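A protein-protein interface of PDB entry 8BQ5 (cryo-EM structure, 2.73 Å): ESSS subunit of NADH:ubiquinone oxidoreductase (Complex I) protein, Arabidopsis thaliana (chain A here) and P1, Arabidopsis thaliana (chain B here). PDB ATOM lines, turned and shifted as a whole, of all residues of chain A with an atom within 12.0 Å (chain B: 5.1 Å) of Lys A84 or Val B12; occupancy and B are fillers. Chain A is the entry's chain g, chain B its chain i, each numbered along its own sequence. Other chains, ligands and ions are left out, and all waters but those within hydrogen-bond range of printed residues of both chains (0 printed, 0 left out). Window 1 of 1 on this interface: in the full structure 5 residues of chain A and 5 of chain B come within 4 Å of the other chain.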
ATOM      1  N   ILE A  74      12.368   9.583 -24.836  1.00  0.00           N
ATOM      2  CA  ILE A  74      13.799   9.298 -24.903  1.00  0.00           C
ATOM      3  C   ILE A  74      14.401   9.865 -26.183  1.00  0.00           C
ATOM      4  O   ILE A  74      15.506  10.418 -26.177  1.00  0.00           O
ATOM      5  CB  ILE A  74      14.050   7.784 -24.779  1.00  0.00           C
ATOM      6  CG1 ILE A  74      13.386   7.234 -23.515  1.00  0.00           C
ATOM      7  CG2 ILE A  74      15.539   7.486 -24.779  1.00  0.00           C
ATOM      8  CD1 ILE A  74      14.261   7.268 -22.283  1.00  0.00           C
ATOM      9  N   VAL A  75      13.688   9.732 -27.304  1.00  0.00           N
ATOM     10  CA  VAL A  75      14.243  10.163 -28.586  1.00  0.00           C
ATOM     11  C   VAL A  75      14.220  11.687 -28.704  1.00  0.00           C
ATOM     12  O   VAL A  75      15.147  12.292 -29.254  1.00  0.00           O
ATOM     13  CB  VAL A  75      13.510   9.475 -29.756  1.00  0.00           C
ATOM     14  CG1 VAL A  75      12.174  10.138 -30.062  1.00  0.00           C
ATOM     15  CG2 VAL A  75      14.389   9.470 -30.993  1.00  0.00           C
ATOM     16  N   ILE A  76      13.168  12.330 -28.192  1.00  0.00           N
ATOM     17  CA  ILE A  76      13.062  13.785 -28.300  1.00  0.00           C
ATOM     18  C   ILE A  76      14.090  14.458 -27.399  1.00  0.00           C
ATOM     19  O   ILE A  76      14.624  15.525 -27.721  1.00  0.00           O
ATOM     20  CB  ILE A  76      11.630  14.251 -27.979  1.00  0.00           C
ATOM     21  CG1 ILE A  76      10.640  13.683 -29.001  1.00  0.00           C
ATOM     22  CG2 ILE A  76      11.543  15.774 -27.935  1.00  0.00           C
ATOM     23  CD1 ILE A  76      10.294  14.627 -30.135  1.00  0.00           C
ATOM     24  N   LEU A  77      14.387  13.838 -26.256  1.00  0.00           N
ATOM     25  CA  LEU A  77      15.330  14.433 -25.314  1.00  0.00           C
ATOM     26  C   LEU A  77      16.745  13.918 -25.547  1.00  0.00           C
ATOM     27  O   LEU A  77      17.713  14.683 -25.474  1.00  0.00           O
ATOM     28  CB  LEU A  77      14.885  14.152 -23.879  1.00  0.00           C
ATOM     29  CG  LEU A  77      13.678  14.944 -23.378  1.00  0.00           C
ATOM     30  CD1 LEU A  77      13.407  14.634 -21.916  1.00  0.00           C
ATOM     31  CD2 LEU A  77      13.907  16.433 -23.578  1.00  0.00           C
ATOM     32  N   GLY A  78      16.889  12.620 -25.818  1.00  0.00           N
ATOM     33  CA  GLY A  78      18.214  12.063 -26.027  1.00  0.00           C
ATOM     34  C   GLY A  78      18.895  12.591 -27.273  1.00  0.00           C
ATOM     35  O   GLY A  78      20.114  12.776 -27.289  1.00  0.00           O
ATOM     36  N   VAL A  79      18.125  12.837 -28.327  1.00  0.00           N
ATOM     37  CA  VAL A  79      18.664  13.380 -29.570  1.00  0.00           C
ATOM     38  C   VAL A  79      18.498  14.892 -29.629  1.00  0.00           C
ATOM     39  O   VAL A  79      19.379  15.607 -30.113  1.00  0.00           O
ATOM     40  CB  VAL A  79      17.989  12.686 -30.773  1.00  0.00           C
ATOM     41  CG1 VAL A  79      18.324  13.401 -32.077  1.00  0.00           C
ATOM     42  CG2 VAL A  79      18.405  11.226 -30.838  1.00  0.00           C
ATOM     43  N   GLY A  80      17.368  15.400 -29.137  1.00  0.00           N
ATOM     44  CA  GLY A  80      17.116  16.830 -29.215  1.00  0.00           C
ATOM     45  C   GLY A  80      18.060  17.654 -28.360  1.00  0.00           C
ATOM     46  O   GLY A  80      18.543  18.705 -28.793  1.00  0.00           O
ATOM     47  N   LEU A  81      18.328  17.203 -27.134  1.00  0.00           N
ATOM     48  CA  LEU A  81      19.190  17.973 -26.244  1.00  0.00           C
ATOM     49  C   LEU A  81      20.630  17.982 -26.743  1.00  0.00           C
ATOM     50  O   LEU A  81      21.338  18.984 -26.593  1.00  0.00           O
ATOM     51  CB  LEU A  81      19.116  17.416 -24.822  1.00  0.00           C
ATOM     52  CG  LEU A  81      17.821  17.666 -24.044  1.00  0.00           C
ATOM     53  CD1 LEU A  81      17.940  17.132 -22.626  1.00  0.00           C
ATOM     54  CD2 LEU A  81      17.450  19.138 -24.039  1.00  0.00           C
ATOM     55  N   ASN A  82      21.079  16.876 -27.337  1.00  0.00           N
ATOM     56  CA  ASN A  82      22.433  16.774 -27.869  1.00  0.00           C
ATOM     57  C   ASN A  82      22.600  17.458 -29.216  1.00  0.00           C
ATOM     58  O   ASN A  82      23.739  17.699 -29.632  1.00  0.00           O
ATOM     59  CB  ASN A  82      22.833  15.304 -28.001  1.00  0.00           C
ATOM     60  CG  ASN A  82      23.015  14.632 -26.662  1.00  0.00           C
ATOM     61  OD1 ASN A  82      24.005  14.858 -25.970  1.00  0.00           O
ATOM     62  ND2 ASN A  82      22.051  13.801 -26.283  1.00  0.00           N
ATOM     63  N   ALA A  83      21.508  17.769 -29.912  1.00  0.00           N
ATOM     64  CA  ALA A  83      21.586  18.401 -31.219  1.00  0.00           C
ATOM     65  C   ALA A  83      21.317  19.895 -31.182  1.00  0.00           C
ATOM     66  O   ALA A  83      21.673  20.596 -32.136  1.00  0.00           O
ATOM     67  CB  ALA A  83      20.597  17.748 -32.186  1.00  0.00           C
ATOM     68  N   LYS A  84      20.683  20.394 -30.128  1.00  0.00           N
ATOM     69  CA  LYS A  84      20.456  21.820 -30.019  1.00  0.00           C
ATOM     70  C   LYS A  84      21.789  22.540 -29.816  1.00  0.00           C
ATOM     71  O   LYS A  84      22.710  21.997 -29.199  1.00  0.00           O
ATOM     72  CB  LYS A  84      19.498  22.121 -28.870  1.00  0.00           C
ATOM     73  CG  LYS A  84      20.063  21.852 -27.488  1.00  0.00           C
ATOM     74  CD  LYS A  84      19.074  22.219 -26.392  1.00  0.00           C
ATOM     75  CE  LYS A  84      18.384  23.541 -26.669  1.00  0.00           C
ATOM     76  NZ  LYS A  84      17.884  24.168 -25.416  1.00  0.00           N
ATOM     77  N   PRO A  85      21.930  23.749 -30.355  1.00  0.00           N
ATOM     78  CA  PRO A  85      23.202  24.466 -30.220  1.00  0.00           C
ATOM     79  C   PRO A  85      23.485  24.829 -28.772  1.00  0.00           C
ATOM     80  O   PRO A  85      22.573  25.073 -27.980  1.00  0.00           O
ATOM     81  CB  PRO A  85      22.997  25.714 -31.083  1.00  0.00           C
ATOM     82  CG  PRO A  85      21.524  25.921 -31.091  1.00  0.00           C
ATOM     83  CD  PRO A  85      20.915  24.550 -31.061  1.00  0.00           C
ATOM     84  N   ASP A  86      24.769  24.859 -28.429  1.00  0.00           N
ATOM     85  CA  ASP A  86      25.189  25.255 -27.090  1.00  0.00           C
ATOM     86  C   ASP A  86      25.204  26.774 -27.012  1.00  0.00           C
ATOM     87  O   ASP A  86      26.230  27.410 -27.275  1.00  0.00           O
ATOM     88  CB  ASP A  86      26.558  24.673 -26.753  1.00  0.00           C
ATOM     89  CG  ASP A  86      26.779  24.551 -25.260  1.00  0.00           C
ATOM     90  OD1 ASP A  86      26.755  25.591 -24.569  1.00  0.00           O
ATOM     91  OD2 ASP A  86      26.960  23.417 -24.777  1.00  0.00           O
ATOM     92  N   LEU A  87      24.063  27.356 -26.647  1.00  0.00           N
ATOM     93  CA  LEU A  87      23.912  28.801 -26.555  1.00  0.00           C
ATOM     94  C   LEU A  87      23.972  29.296 -25.117  1.00  0.00           C
ATOM     95  O   LEU A  87      23.594  30.437 -24.843  1.00  0.00           O
ATOM     96  CB  LEU A  87      22.603  29.234 -27.216  1.00  0.00           C
ATOM     97  CG  LEU A  87      22.378  28.645 -28.609  1.00  0.00           C
ATOM     98  CD1 LEU A  87      20.979  28.957 -29.115  1.00  0.00           C
ATOM     99  CD2 LEU A  87      23.434  29.145 -29.583  1.00  0.00           C
ATOM    100  N   SER A  88      24.442  28.463 -24.193  1.00  0.00           N
ATOM    101  CA  SER A  88      24.531  28.874 -22.799  1.00  0.00           C
ATOM    102  C   SER A  88      25.486  30.053 -22.651  1.00  0.00           C
ATOM    103  O   SER A  88      26.470  30.184 -23.386  1.00  0.00           O
ATOM    104  CB  SER A  88      24.991  27.706 -21.928  1.00  0.00           C
ATOM    105  OG  SER A  88      26.350  27.395 -22.173  1.00  0.00           O
ATOM    106  N   ILE A  89      25.175  30.929 -21.691  1.00  0.00           N
ATOM    107  CA  ILE A  89      25.984  32.128 -21.478  1.00  0.00           C
ATOM    108  C   ILE A  89      27.414  31.760 -21.117  1.00  0.00           C
ATOM    109  O   ILE A  89      28.363  32.427 -21.548  1.00  0.00           O
ATOM    110  CB  ILE A  89      25.339  33.025 -20.399  1.00  0.00           C
ATOM    111  CG1 ILE A  89      26.287  34.155 -19.998  1.00  0.00           C
ATOM    112  CG2 ILE A  89      24.938  32.206 -19.180  1.00  0.00           C
ATOM    113  CD1 ILE A  89      26.386  35.263 -21.014  1.00  0.00           C
ATOM    114  N   GLU A  90      27.596  30.691 -20.342  1.00  0.00           N
ATOM    115  CA  GLU A  90      28.934  30.289 -19.922  1.00  0.00           C
ATOM    116  C   GLU A  90      29.813  29.955 -21.121  1.00  0.00           C
ATOM    117  O   GLU A  90      30.982  30.352 -21.176  1.00  0.00           O
ATOM    118  CB  GLU A  90      28.839  29.100 -18.965  1.00  0.00           C
ATOM    119  CG  GLU A  90      27.939  29.346 -17.761  1.00  0.00           C
ATOM    120  CD  GLU A  90      26.600  28.633 -17.857  1.00  0.00           C
ATOM    121  OE1 GLU A  90      26.042  28.274 -16.800  1.00  0.00           O
ATOM    122  OE2 GLU A  90      26.101  28.434 -18.983  1.00  0.00           O
ATOM    123  N   THR A  91      29.266  29.234 -22.101  1.00  0.00           N
ATOM    124  CA  THR A  91      30.053  28.891 -23.282  1.00  0.00           C
ATOM    125  C   THR A  91      30.471  30.140 -24.050  1.00  0.00           C
ATOM    126  O   THR A  91      31.606  30.228 -24.534  1.00  0.00           O
ATOM    127  CB  THR A  91      29.262  27.947 -24.186  1.00  0.00           C
ATOM    128  OG1 THR A  91      28.883  26.781 -23.445  1.00  0.00           O
ATOM    129  CG2 THR A  91      30.102  27.523 -25.379  1.00  0.00           C
ATOM    130  N   ALA B   8      19.602  16.449 -37.343  1.00  0.00           N
ATOM    131  CA  ALA B   8      18.962  16.934 -36.127  1.00  0.00           C
ATOM    132  C   ALA B   8      19.293  18.400 -35.866  1.00  0.00           C
ATOM    133  O   ALA B   8      18.415  19.175 -35.468  1.00  0.00           O
ATOM    134  CB  ALA B   8      19.368  16.061 -34.941  1.00  0.00           C
ATOM    135  N   GLU B   9      20.549  18.805 -36.094  1.00  0.00           N
ATOM    136  CA  GLU B   9      20.929  20.199 -35.870  1.00  0.00           C
ATOM    137  C   GLU B   9      20.083  21.138 -36.719  1.00  0.00           C
ATOM    138  O   GLU B   9      19.559  22.143 -36.225  1.00  0.00           O
ATOM    139  CB  GLU B   9      22.413  20.426 -36.181  1.00  0.00           C
ATOM    140  CG  GLU B   9      23.333  19.233 -36.008  1.00  0.00           C
ATOM    141  CD  GLU B   9      23.704  18.972 -34.561  1.00  0.00           C
ATOM    142  OE1 GLU B   9      23.959  19.943 -33.818  1.00  0.00           O
ATOM    143  OE2 GLU B   9      23.744  17.789 -34.167  1.00  0.00           O
ATOM    144  N   ASN B  10      19.938  20.820 -38.006  1.00  0.00           N
ATOM    145  CA  ASN B  10      19.164  21.678 -38.895  1.00  0.00           C
ATOM    146  C   ASN B  10      17.707  21.746 -38.462  1.00  0.00           C
ATOM    147  O   ASN B  10      17.113  22.829 -38.433  1.00  0.00           O
ATOM    148  CB  ASN B  10      19.277  21.176 -40.333  1.00  0.00           C
ATOM    149  CG  ASN B  10      20.267  21.975 -41.150  1.00  0.00           C
ATOM    150  OD1 ASN B  10      19.882  22.814 -41.963  1.00  0.00           O
ATOM    151  ND2 ASN B  10      21.554  21.727 -40.930  1.00  0.00           N
ATOM    152  N   LEU B  11      17.123  20.601 -38.103  1.00  0.00           N
ATOM    153  CA  LEU B  11      15.734  20.586 -37.660  1.00  0.00           C
ATOM    154  C   LEU B  11      15.544  21.436 -36.412  1.00  0.00           C
ATOM    155  O   LEU B  11      14.592  22.219 -36.325  1.00  0.00           O
ATOM    156  CB  LEU B  11      15.282  19.150 -37.402  1.00  0.00           C
ATOM    157  CG  LEU B  11      13.794  18.949 -37.121  1.00  0.00           C
ATOM    158  CD1 LEU B  11      12.978  19.127 -38.387  1.00  0.00           C
ATOM    159  CD2 LEU B  11      13.550  17.580 -36.508  1.00  0.00           C
ATOM    160  N   VAL B  12      16.447  21.301 -35.438  1.00  0.00           N
ATOM    161  CA  VAL B  12      16.374  22.132 -34.241  1.00  0.00           C
ATOM    162  C   VAL B  12      16.513  23.601 -34.613  1.00  0.00           C
ATOM    163  O   VAL B  12      15.831  24.468 -34.056  1.00  0.00           O
ATOM    164  CB  VAL B  12      17.447  21.697 -33.224  1.00  0.00           C
ATOM    165  CG1 VAL B  12      17.497  22.664 -32.051  1.00  0.00           C
ATOM    166  CG2 VAL B  12      17.180  20.281 -32.738  1.00  0.00           C
ATOM    167  N   LEU B  13      17.379  23.898 -35.586  1.00  0.00           N
ATOM    168  CA  LEU B  13      17.630  25.284 -35.967  1.00  0.00           C
ATOM    169  C   LEU B  13      16.399  25.928 -36.599  1.00  0.00           C
ATOM    170  O   LEU B  13      16.155  27.125 -36.408  1.00  0.00           O
ATOM    171  CB  LEU B  13      18.828  25.351 -36.914  1.00  0.00           C
ATOM    172  CG  LEU B  13      20.210  25.381 -36.252  1.00  0.00           C
ATOM    173  CD1 LEU B  13      21.261  25.878 -37.223  1.00  0.00           C
ATOM    174  CD2 LEU B  13      20.193  26.243 -35.000  1.00  0.00           C
ATOM    175  N   ARG B  14      15.611  25.160 -37.360  1.00  0.00           N
ATOM    176  CA  ARG B  14      14.397  25.724 -37.948  1.00  0.00           C
ATOM    177  C   ARG B  14      13.329  25.978 -36.891  1.00  0.00           C
ATOM    178  O   ARG B  14      12.406  26.770 -37.112  1.00  0.00           O
ATOM    179  CB  ARG B  14      13.829  24.814 -39.040  1.00  0.00           C
ATOM    180  CG  ARG B  14      14.658  24.661 -40.294  1.00  0.00           C
ATOM    181  CD  ARG B  14      13.937  23.770 -41.295  1.00  0.00           C
ATOM    182  NE  ARG B  14      14.735  23.540 -42.494  1.00  0.00           N
ATOM    183  CZ  ARG B  14      14.400  22.713 -43.474  1.00  0.00           C
ATOM    184  NH1 ARG B  14      13.280  22.009 -43.432  1.00  0.00           N
ATOM    185  NH2 ARG B  14      15.210  22.583 -44.521  1.00  0.00           N
ATOM    186  N   LEU B  15      13.424  25.304 -35.744  1.00  0.00           N
ATOM    187  CA  LEU B  15      12.394  25.437 -34.722  1.00  0.00           C
ATOM    188  C   LEU B  15      12.650  26.602 -33.776  1.00  0.00           C
ATOM    189  O   LEU B  15      11.753  26.966 -33.011  1.00  0.00           O
ATOM    190  CB  LEU B  15      12.283  24.143 -33.917  1.00  0.00           C
ATOM    191  CG  LEU B  15      11.977  22.869 -34.704  1.00  0.00           C
ATOM    192  CD1 LEU B  15      12.447  21.657 -33.924  1.00  0.00           C
ATOM    193  CD2 LEU B  15      10.499  22.760 -35.040  1.00  0.00           C
ATOM    194  N   MET B  16      13.842  27.191 -33.807  1.00  0.00           N
ATOM    195  CA  MET B  16      14.172  28.258 -32.873  1.00  0.00           C
ATOM    196  C   MET B  16      13.869  29.617 -33.489  1.00  0.00           C
ATOM    197  O   MET B  16      14.246  29.892 -34.631  1.00  0.00           O
ATOM    198  CB  MET B  16      15.645  28.176 -32.480  1.00  0.00           C
ATOM    199  CG  MET B  16      16.073  26.809 -31.985  1.00  0.00           C
ATOM    200  SD  MET B  16      17.824  26.703 -31.574  1.00  0.00           S
ATOM    201  CE  MET B  16      17.782  27.046 -29.820  1.00  0.00           C
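The backbone carbonyl oxygen (O) of Ala A83 sits close to the side-chain carboxylate (OE1) of Glu B9 (2.9 Å).
Printed residues of chain B within 4 Å of Ala A83: Ala B8 and Glu B9.
Printed residues of chain B within 4 Å of Pro A85: Met B16.
Of the printed residues of chain B, Leu A87 touches Met B16.
Ala B8 touches just one residue of chain A: Ala A83 (3.5 Å).
No residue of chain A comes within 4 Å of Asn B10.
Leu B11 touches none of the printed residues of chain A.
Of chain A, only Lys A84 (3.7 Å) comes within 4 Å of Val B12.
No residue of chain A comes within 4 Å of Leu B15.
Of the printed residues of chain A, Met B16 touches Pro A85 and Leu A87.
The nearest residue of chain A that does not touch Val B12 is Pro A85 (4.03 Å).
Among the printed residues, merely in contact across the chains: Ala A83 with Ala B8 (3.5 Å), Lys A84 with Val B12 (3.7 Å), Pro A85 with Met B16 (3.8 Å) and Leu A87 with Met B16 (3.8 Å).
Of the 9 printed residues of chain B, 4 touch a printed residue of chain A.
Hydrophobic or aromatic side chains of chain B that line the printed part of chain A: Ala B8, Val B12 and Met B16.
Of the 18 printed residues of chain A, 4 touch a printed residue of chain B.
Hydrophobic or aromatic side chains of chain A that line the printed part of chain B: Ala A83, Pro A85 and Leu A87.
Among the printed residues, 5 pairs touch across the chains.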
